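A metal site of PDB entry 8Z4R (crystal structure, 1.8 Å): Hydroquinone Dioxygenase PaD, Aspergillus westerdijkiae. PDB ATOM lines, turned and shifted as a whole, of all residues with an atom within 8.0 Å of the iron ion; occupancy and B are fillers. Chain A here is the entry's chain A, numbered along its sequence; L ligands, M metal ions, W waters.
The backbone NH (N) of His 61 sits at hydrogen-bond distance from an oxygen (O2) of the ligand (2.8 Å). A ring nitrogen (ND1) of His 61 lies within hydrogen-bond range of an oxygen (O2) of the ligand (2.8 Å).
A ring nitrogen (ND1) of His 166 lies within hydrogen-bond range of the backbone carbonyl oxygen (O) of Tyr 164, 3.4 Å away. A ring nitrogen (ND1) of His 166 sits at hydrogen-bond distance from a ring nitrogen (ND1) of His 61 (3.5 Å). A ring nitrogen (ND1) of His 166 lies within hydrogen-bond range of the backbone carbonyl oxygen (O) of Gly 163 (2.7 Å). A ring nitrogen (ND1) of His 66 sits at hydrogen-bond distance from NZ of KCX 397, 3.2 Å away. OQ1 of KCX 397 lies within hydrogen-bond range of the side-chain hydroxyl (OG1) of Thr 320. ND1 of His 317 lies within hydrogen-bond range of O of Phe 313 (2.8 Å). A ring nitrogen (ND1) of His 394 is in hydrogen-bond range of the side-chain carboxylate (OD1) of Asp 392 (2.7 Å). O of His 61 sits at hydrogen-bond distance from ND1 of His 63 (2.9 Å).
Of the 20 residues printed, 5 come within 4 Å of the iron ion. The nearest printed residue that does not touch the iron ion is Phe 313 (4.7 Å).
The iron ion is bound by a ring nitrogen (NE2) of His 166 (2.0 Å), OQ2 of KCX 397 (2.1 Å), a ring nitrogen (NE2) of His 317 (2.1 Å), a ring nitrogen (NE2) of His 394 (2.1 Å), a ring nitrogen (NE2) of His 63 (2.2 Å) and water W1 (2.3 Å).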
ATOM      1  N   PHE A  60      33.481 -18.881  13.779  1.00  0.00           N
ATOM      2  CA  PHE A  60      32.180 -18.312  14.187  1.00  0.00           C
ATOM      3  C   PHE A  60      32.481 -17.059  15.031  1.00  0.00           C
ATOM      4  O   PHE A  60      33.502 -17.022  15.677  1.00  0.00           O
ATOM      5  CB  PHE A  60      31.314 -19.297  14.974  1.00  0.00           C
ATOM      6  CG  PHE A  60      30.700 -20.417  14.171  1.00  0.00           C
ATOM      7  CD1 PHE A  60      31.073 -20.698  12.873  1.00  0.00           C
ATOM      8  CD2 PHE A  60      29.726 -21.217  14.768  1.00  0.00           C
ATOM      9  CE1 PHE A  60      30.458 -21.706  12.143  1.00  0.00           C
ATOM     10  CE2 PHE A  60      29.107 -22.225  14.048  1.00  0.00           C
ATOM     11  CZ  PHE A  60      29.480 -22.470  12.738  1.00  0.00           C
ATOM     12  N   HIS A  61      31.658 -16.030  14.864  1.00  0.00           N
ATOM     13  CA  HIS A  61      31.910 -14.689  15.477  1.00  0.00           C
ATOM     14  C   HIS A  61      31.118 -14.455  16.749  1.00  0.00           C
ATOM     15  O   HIS A  61      30.008 -14.905  16.864  1.00  0.00           O
ATOM     16  CB  HIS A  61      31.696 -13.553  14.436  1.00  0.00           C
ATOM     17  CG  HIS A  61      32.554 -13.659  13.241  1.00  0.00           C
ATOM     18  ND1 HIS A  61      32.294 -14.565  12.237  1.00  0.00           N
ATOM     19  CD2 HIS A  61      33.639 -12.973  12.847  1.00  0.00           C
ATOM     20  CE1 HIS A  61      33.202 -14.448  11.314  1.00  0.00           C
ATOM     21  NE2 HIS A  61      34.018 -13.506  11.649  1.00  0.00           N
ATOM     22  N   ASN A  62      31.726 -13.713  17.649  1.00  0.00           N
ATOM     23  CA  ASN A  62      31.061 -13.205  18.858  1.00  0.00           C
ATOM     24  C   ASN A  62      30.165 -12.030  18.460  1.00  0.00           C
ATOM     25  O   ASN A  62      30.721 -10.976  18.015  1.00  0.00           O
ATOM     26  CB  ASN A  62      32.096 -12.831  19.900  1.00  0.00           C
ATOM     27  CG  ASN A  62      31.448 -12.275  21.136  1.00  0.00           C
ATOM     28  OD1 ASN A  62      30.224 -12.354  21.269  1.00  0.00           O
ATOM     29  ND2 ASN A  62      32.286 -11.803  22.061  1.00  0.00           N
ATOM     30  N   HIS A  63      28.865 -12.214  18.566  1.00  0.00           N
ATOM     31  CA  HIS A  63      27.873 -11.201  18.176  1.00  0.00           C
ATOM     32  C   HIS A  63      27.350 -10.450  19.393  1.00  0.00           C
ATOM     33  O   HIS A  63      26.340  -9.711  19.266  1.00  0.00           O
ATOM     34  CB  HIS A  63      26.699 -11.740  17.426  1.00  0.00           C
ATOM     35  CG  HIS A  63      27.076 -12.204  16.067  1.00  0.00           C
ATOM     36  ND1 HIS A  63      27.823 -13.353  15.855  1.00  0.00           N
ATOM     37  CD2 HIS A  63      26.750 -11.715  14.853  1.00  0.00           C
ATOM     38  CE1 HIS A  63      27.944 -13.533  14.547  1.00  0.00           C
ATOM     39  NE2 HIS A  63      27.383 -12.503  13.923  1.00  0.00           N
ATOM     40  N   HIS A  66      27.056  -6.585  19.200  1.00  0.00           N
ATOM     41  CA  HIS A  66      25.987  -6.206  18.244  1.00  0.00           C
ATOM     42  C   HIS A  66      24.592  -6.470  18.807  1.00  0.00           C
ATOM     43  O   HIS A  66      23.688  -5.647  18.644  1.00  0.00           O
ATOM     44  CB  HIS A  66      26.078  -6.986  16.921  1.00  0.00           C
ATOM     45  CG  HIS A  66      27.431  -7.216  16.380  1.00  0.00           C
ATOM     46  ND1 HIS A  66      27.658  -8.136  15.365  1.00  0.00           N
ATOM     47  CD2 HIS A  66      28.594  -6.571  16.560  1.00  0.00           C
ATOM     48  CE1 HIS A  66      28.943  -8.116  15.053  1.00  0.00           C
ATOM     49  NE2 HIS A  66      29.541  -7.185  15.787  1.00  0.00           N
ATOM     50  N   GLY A 163      35.537 -12.801   6.797  1.00  0.00           N
ATOM     51  CA  GLY A 163      34.690 -13.409   7.834  1.00  0.00           C
ATOM     52  C   GLY A 163      33.288 -12.905   7.724  1.00  0.00           C
ATOM     53  O   GLY A 163      32.719 -12.686   8.758  1.00  0.00           O
ATOM     54  N   TYR A 164      32.711 -12.819   6.506  1.00  0.00           N
ATOM     55  CA  TYR A 164      31.302 -12.404   6.288  1.00  0.00           C
ATOM     56  C   TYR A 164      31.088 -11.000   6.887  1.00  0.00           C
ATOM     57  O   TYR A 164      30.046 -10.721   7.479  1.00  0.00           O
ATOM     58  CB  TYR A 164      30.315 -13.478   6.786  1.00  0.00           C
ATOM     59  CG  TYR A 164      30.713 -14.866   6.330  1.00  0.00           C
ATOM     60  CD1 TYR A 164      31.211 -15.811   7.229  1.00  0.00           C
ATOM     61  CD2 TYR A 164      30.738 -15.186   4.978  1.00  0.00           C
ATOM     62  CE1 TYR A 164      31.666 -17.043   6.803  1.00  0.00           C
ATOM     63  CE2 TYR A 164      31.197 -16.417   4.542  1.00  0.00           C
ATOM     64  CZ  TYR A 164      31.637 -17.365   5.452  1.00  0.00           C
ATOM     65  OH  TYR A 164      32.124 -18.578   5.048  1.00  0.00           O
ATOM     66  N   VAL A 165      32.051 -10.115   6.648  1.00  0.00           N
ATOM     67  CA  VAL A 165      31.917  -8.630   6.828  1.00  0.00           C
ATOM     68  C   VAL A 165      31.682  -8.244   8.294  1.00  0.00           C
ATOM     69  O   VAL A 165      31.150  -7.151   8.544  1.00  0.00           O
ATOM     70  CB  VAL A 165      30.878  -7.983   5.860  1.00  0.00           C
ATOM     71  CG1 VAL A 165      31.204  -8.363   4.438  1.00  0.00           C
ATOM     72  CG2 VAL A 165      29.429  -8.278   6.114  1.00  0.00           C
ATOM     73  N   HIS A 166      32.103  -9.056   9.270  1.00  0.00           N
ATOM     74  CA  HIS A 166      31.869  -8.698  10.683  1.00  0.00           C
ATOM     75  C   HIS A 166      32.730  -7.470  11.075  1.00  0.00           C
ATOM     76  O   HIS A 166      32.258  -6.722  11.927  1.00  0.00           O
ATOM     77  CB  HIS A 166      31.962  -9.934  11.616  1.00  0.00           C
ATOM     78  CG  HIS A 166      30.803 -10.835  11.441  1.00  0.00           C
ATOM     79  ND1 HIS A 166      30.839 -11.891  10.559  1.00  0.00           N
ATOM     80  CD2 HIS A 166      29.545 -10.842  11.988  1.00  0.00           C
ATOM     81  CE1 HIS A 166      29.652 -12.474  10.562  1.00  0.00           C
ATOM     82  NE2 HIS A 166      28.807 -11.857  11.426  1.00  0.00           N
ATOM     83  N   ILE A 169      30.764  -4.373  10.003  1.00  0.00           N
ATOM     84  CA  ILE A 169      29.574  -4.322  10.873  1.00  0.00           C
ATOM     85  C   ILE A 169      29.980  -3.671  12.211  1.00  0.00           C
ATOM     86  O   ILE A 169      29.272  -2.752  12.685  1.00  0.00           O
ATOM     87  CB  ILE A 169      28.932  -5.697  11.076  1.00  0.00           C
ATOM     88  CG1 ILE A 169      28.284  -6.199   9.774  1.00  0.00           C
ATOM     89  CG2 ILE A 169      27.922  -5.682  12.226  1.00  0.00           C
ATOM     90  CD1 ILE A 169      27.829  -7.651   9.844  1.00  0.00           C
ATOM     91  N   PHE A 313      20.775 -16.643   6.020  1.00  0.00           N
ATOM     92  CA  PHE A 313      21.739 -16.277   7.089  1.00  0.00           C
ATOM     93  C   PHE A 313      22.921 -15.516   6.474  1.00  0.00           C
ATOM     94  O   PHE A 313      23.509 -14.603   7.088  1.00  0.00           O
ATOM     95  CB  PHE A 313      22.221 -17.543   7.783  1.00  0.00           C
ATOM     96  CG  PHE A 313      23.154 -17.247   8.915  1.00  0.00           C
ATOM     97  CD1 PHE A 313      22.638 -16.759  10.105  1.00  0.00           C
ATOM     98  CD2 PHE A 313      24.529 -17.394   8.766  1.00  0.00           C
ATOM     99  CE1 PHE A 313      23.496 -16.425  11.124  1.00  0.00           C
ATOM    100  CE2 PHE A 313      25.389 -17.068   9.796  1.00  0.00           C
ATOM    101  CZ  PHE A 313      24.858 -16.593  10.981  1.00  0.00           C
ATOM    102  N   PHE A 314      23.376 -15.978   5.315  1.00  0.00           N
ATOM    103  CA  PHE A 314      24.560 -15.394   4.628  1.00  0.00           C
ATOM    104  C   PHE A 314      24.115 -14.083   3.990  1.00  0.00           C
ATOM    105  O   PHE A 314      24.811 -13.077   4.195  1.00  0.00           O
ATOM    106  CB  PHE A 314      25.224 -16.368   3.647  1.00  0.00           C
ATOM    107  CG  PHE A 314      25.995 -17.426   4.371  1.00  0.00           C
ATOM    108  CD1 PHE A 314      25.341 -18.558   4.855  1.00  0.00           C
ATOM    109  CD2 PHE A 314      27.297 -17.210   4.756  1.00  0.00           C
ATOM    110  CE1 PHE A 314      26.014 -19.466   5.638  1.00  0.00           C
ATOM    111  CE2 PHE A 314      27.966 -18.133   5.548  1.00  0.00           C
ATOM    112  CZ  PHE A 314      27.321 -19.278   5.961  1.00  0.00           C
ATOM    113  N   LEU A 316      21.719 -12.017   4.679  1.00  0.00           N
ATOM    114  CA  LEU A 316      21.309 -10.907   5.581  1.00  0.00           C
ATOM    115  C   LEU A 316      22.518 -10.133   6.118  1.00  0.00           C
ATOM    116  O   LEU A 316      22.279  -8.985   6.572  1.00  0.00           O
ATOM    117  CB  LEU A 316      20.392 -11.390   6.697  1.00  0.00           C
ATOM    118  CG  LEU A 316      21.007 -12.306   7.735  1.00  0.00           C
ATOM    119  CD1 LEU A 316      21.752 -11.516   8.792  1.00  0.00           C
ATOM    120  CD2 LEU A 316      19.907 -13.125   8.381  1.00  0.00           C
ATOM    121  N   HIS A 317      23.744 -10.630   6.013  1.00  0.00           N
ATOM    122  CA  HIS A 317      24.924  -9.835   6.389  1.00  0.00           C
ATOM    123  C   HIS A 317      25.059  -8.646   5.402  1.00  0.00           C
ATOM    124  O   HIS A 317      25.738  -7.657   5.772  1.00  0.00           O
ATOM    125  CB  HIS A 317      26.199 -10.682   6.466  1.00  0.00           C
ATOM    126  CG  HIS A 317      26.168 -11.537   7.690  1.00  0.00           C
ATOM    127  ND1 HIS A 317      25.275 -12.583   7.818  1.00  0.00           N
ATOM    128  CD2 HIS A 317      26.784 -11.399   8.899  1.00  0.00           C
ATOM    129  CE1 HIS A 317      25.376 -13.088   9.045  1.00  0.00           C
ATOM    130  NE2 HIS A 317      26.285 -12.382   9.738  1.00  0.00           N
ATOM    131  N   THR A 320      22.676  -6.095   7.200  1.00  0.00           N
ATOM    132  CA  THR A 320      23.220  -5.598   8.496  1.00  0.00           C
ATOM    133  C   THR A 320      24.511  -4.785   8.294  1.00  0.00           C
ATOM    134  O   THR A 320      24.724  -3.906   9.111  1.00  0.00           O
ATOM    135  CB  THR A 320      23.358  -6.719   9.519  1.00  0.00           C
ATOM    136  OG1 THR A 320      24.345  -7.628   9.052  1.00  0.00           O
ATOM    137  CG2 THR A 320      22.003  -7.349   9.759  1.00  0.00           C
ATOM    138  N   ASP A 392      21.280 -14.825  18.573  1.00  0.00           N
ATOM    139  CA  ASP A 392      22.554 -14.151  18.911  1.00  0.00           C
ATOM    140  C   ASP A 392      22.560 -12.720  18.375  1.00  0.00           C
ATOM    141  O   ASP A 392      23.639 -12.100  18.428  1.00  0.00           O
ATOM    142  CB  ASP A 392      23.767 -14.871  18.313  1.00  0.00           C
ATOM    143  CG  ASP A 392      23.651 -15.111  16.811  1.00  0.00           C
ATOM    144  OD1 ASP A 392      22.589 -14.782  16.189  1.00  0.00           O
ATOM    145  OD2 ASP A 392      24.623 -15.718  16.260  1.00  0.00           O
ATOM    146  N   GLY A 393      21.421 -12.252  17.894  1.00  0.00           N
ATOM    147  CA  GLY A 393      21.298 -10.873  17.385  1.00  0.00           C
ATOM    148  C   GLY A 393      20.964 -10.775  15.927  1.00  0.00           C
ATOM    149  O   GLY A 393      20.577  -9.666  15.505  1.00  0.00           O
ATOM    150  N   HIS A 394      21.091 -11.841  15.122  1.00  0.00           N
ATOM    151  CA  HIS A 394      20.897 -11.634  13.661  1.00  0.00           C
ATOM    152  C   HIS A 394      19.473 -11.110  13.372  1.00  0.00           C
ATOM    153  O   HIS A 394      19.380 -10.201  12.474  1.00  0.00           O
ATOM    154  CB  HIS A 394      21.250 -12.883  12.834  1.00  0.00           C
ATOM    155  CG  HIS A 394      22.719 -13.084  12.784  1.00  0.00           C
ATOM    156  ND1 HIS A 394      23.405 -13.820  13.761  1.00  0.00           N
ATOM    157  CD2 HIS A 394      23.670 -12.582  11.948  1.00  0.00           C
ATOM    158  CE1 HIS A 394      24.689 -13.878  13.450  1.00  0.00           C
ATOM    159  NE2 HIS A 394      24.928 -13.038  12.377  1.00  0.00           N
ATOM    160  N   KCX A 397      19.090  -7.347  14.288  1.00  0.00           N
ATOM    161  CA  KCX A 397      19.927  -6.508  13.438  1.00  0.00           C
ATOM    162  CB  KCX A 397      21.390  -6.984  13.314  1.00  0.00           C
ATOM    163  CG  KCX A 397      22.176  -7.026  14.609  1.00  0.00           C
ATOM    164  CD  KCX A 397      23.440  -7.905  14.565  1.00  0.00           C
ATOM    165  CE  KCX A 397      24.384  -7.651  13.398  1.00  0.00           C
ATOM    166  NZ  KCX A 397      25.376  -8.715  13.223  1.00  0.00           N
ATOM    167  C   KCX A 397      19.305  -6.407  12.043  1.00  0.00           C
ATOM    168  O   KCX A 397      19.280  -5.320  11.479  1.00  0.00           O
ATOM    169  CX  KCX A 397      25.493  -9.445  12.047  1.00  0.00           C
ATOM    170  OQ1 KCX A 397      24.806  -9.277  11.086  1.00  0.00           O
ATOM    171  OQ2 KCX A 397      26.367 -10.374  12.019  1.00  0.00           O
ATOM    172  N   HIS A 446      22.131 -22.061  14.230  1.00  0.00           N
ATOM    173  CA  HIS A 446      20.900 -21.332  13.861  1.00  0.00           C
ATOM    174  C   HIS A 446      19.952 -22.282  13.146  1.00  0.00           C
ATOM    175  O   HIS A 446      20.410 -23.035  12.268  1.00  0.00           O
ATOM    176  CB  HIS A 446      21.235 -20.169  12.917  1.00  0.00           C
ATOM    177  CG  HIS A 446      21.762 -18.960  13.590  1.00  0.00           C
ATOM    178  ND1 HIS A 446      20.929 -18.010  14.103  1.00  0.00           N
ATOM    179  CD2 HIS A 446      23.012 -18.559  13.858  1.00  0.00           C
ATOM    180  CE1 HIS A 446      21.661 -17.072  14.642  1.00  0.00           C
ATOM    181  NE2 HIS A 446      22.918 -17.366  14.525  1.00  0.00           N
HETATM  182  C1  LIG L   1      26.589 -18.457  15.003  1.00  0.00           C
HETATM  183  O1  LIG L   1      26.595 -19.053  13.689  1.00  0.00           O
HETATM  184  C2  LIG L   1      27.566 -18.475  12.881  1.00  0.00           C
HETATM  185  C3  LIG L   1      28.274 -17.317  13.217  1.00  0.00           C
HETATM  186  C4  LIG L   1      29.208 -16.840  12.299  1.00  0.00           C
HETATM  187  O2  LIG L   1      29.823 -15.811  12.709  1.00  0.00           O
HETATM  188  C5  LIG L   1      29.521 -17.430  11.078  1.00  0.00           C
HETATM  189  C6  LIG L   1      28.812 -18.602  10.742  1.00  0.00           C
HETATM  190  C7  LIG L   1      29.061 -19.279   9.530  1.00  0.00           C
HETATM  191  C8  LIG L   1      27.848 -19.090  11.659  1.00  0.00           C
HETATM  192  O3  LIG L   1      27.131 -20.198  11.340  1.00  0.00           O
HETATM  193 FE    FE M   1      26.883 -12.382  11.795  1.00  0.00          FE
HETATM  194  O   HOH W   1      27.538 -14.566  11.581  1.00  0.00           O
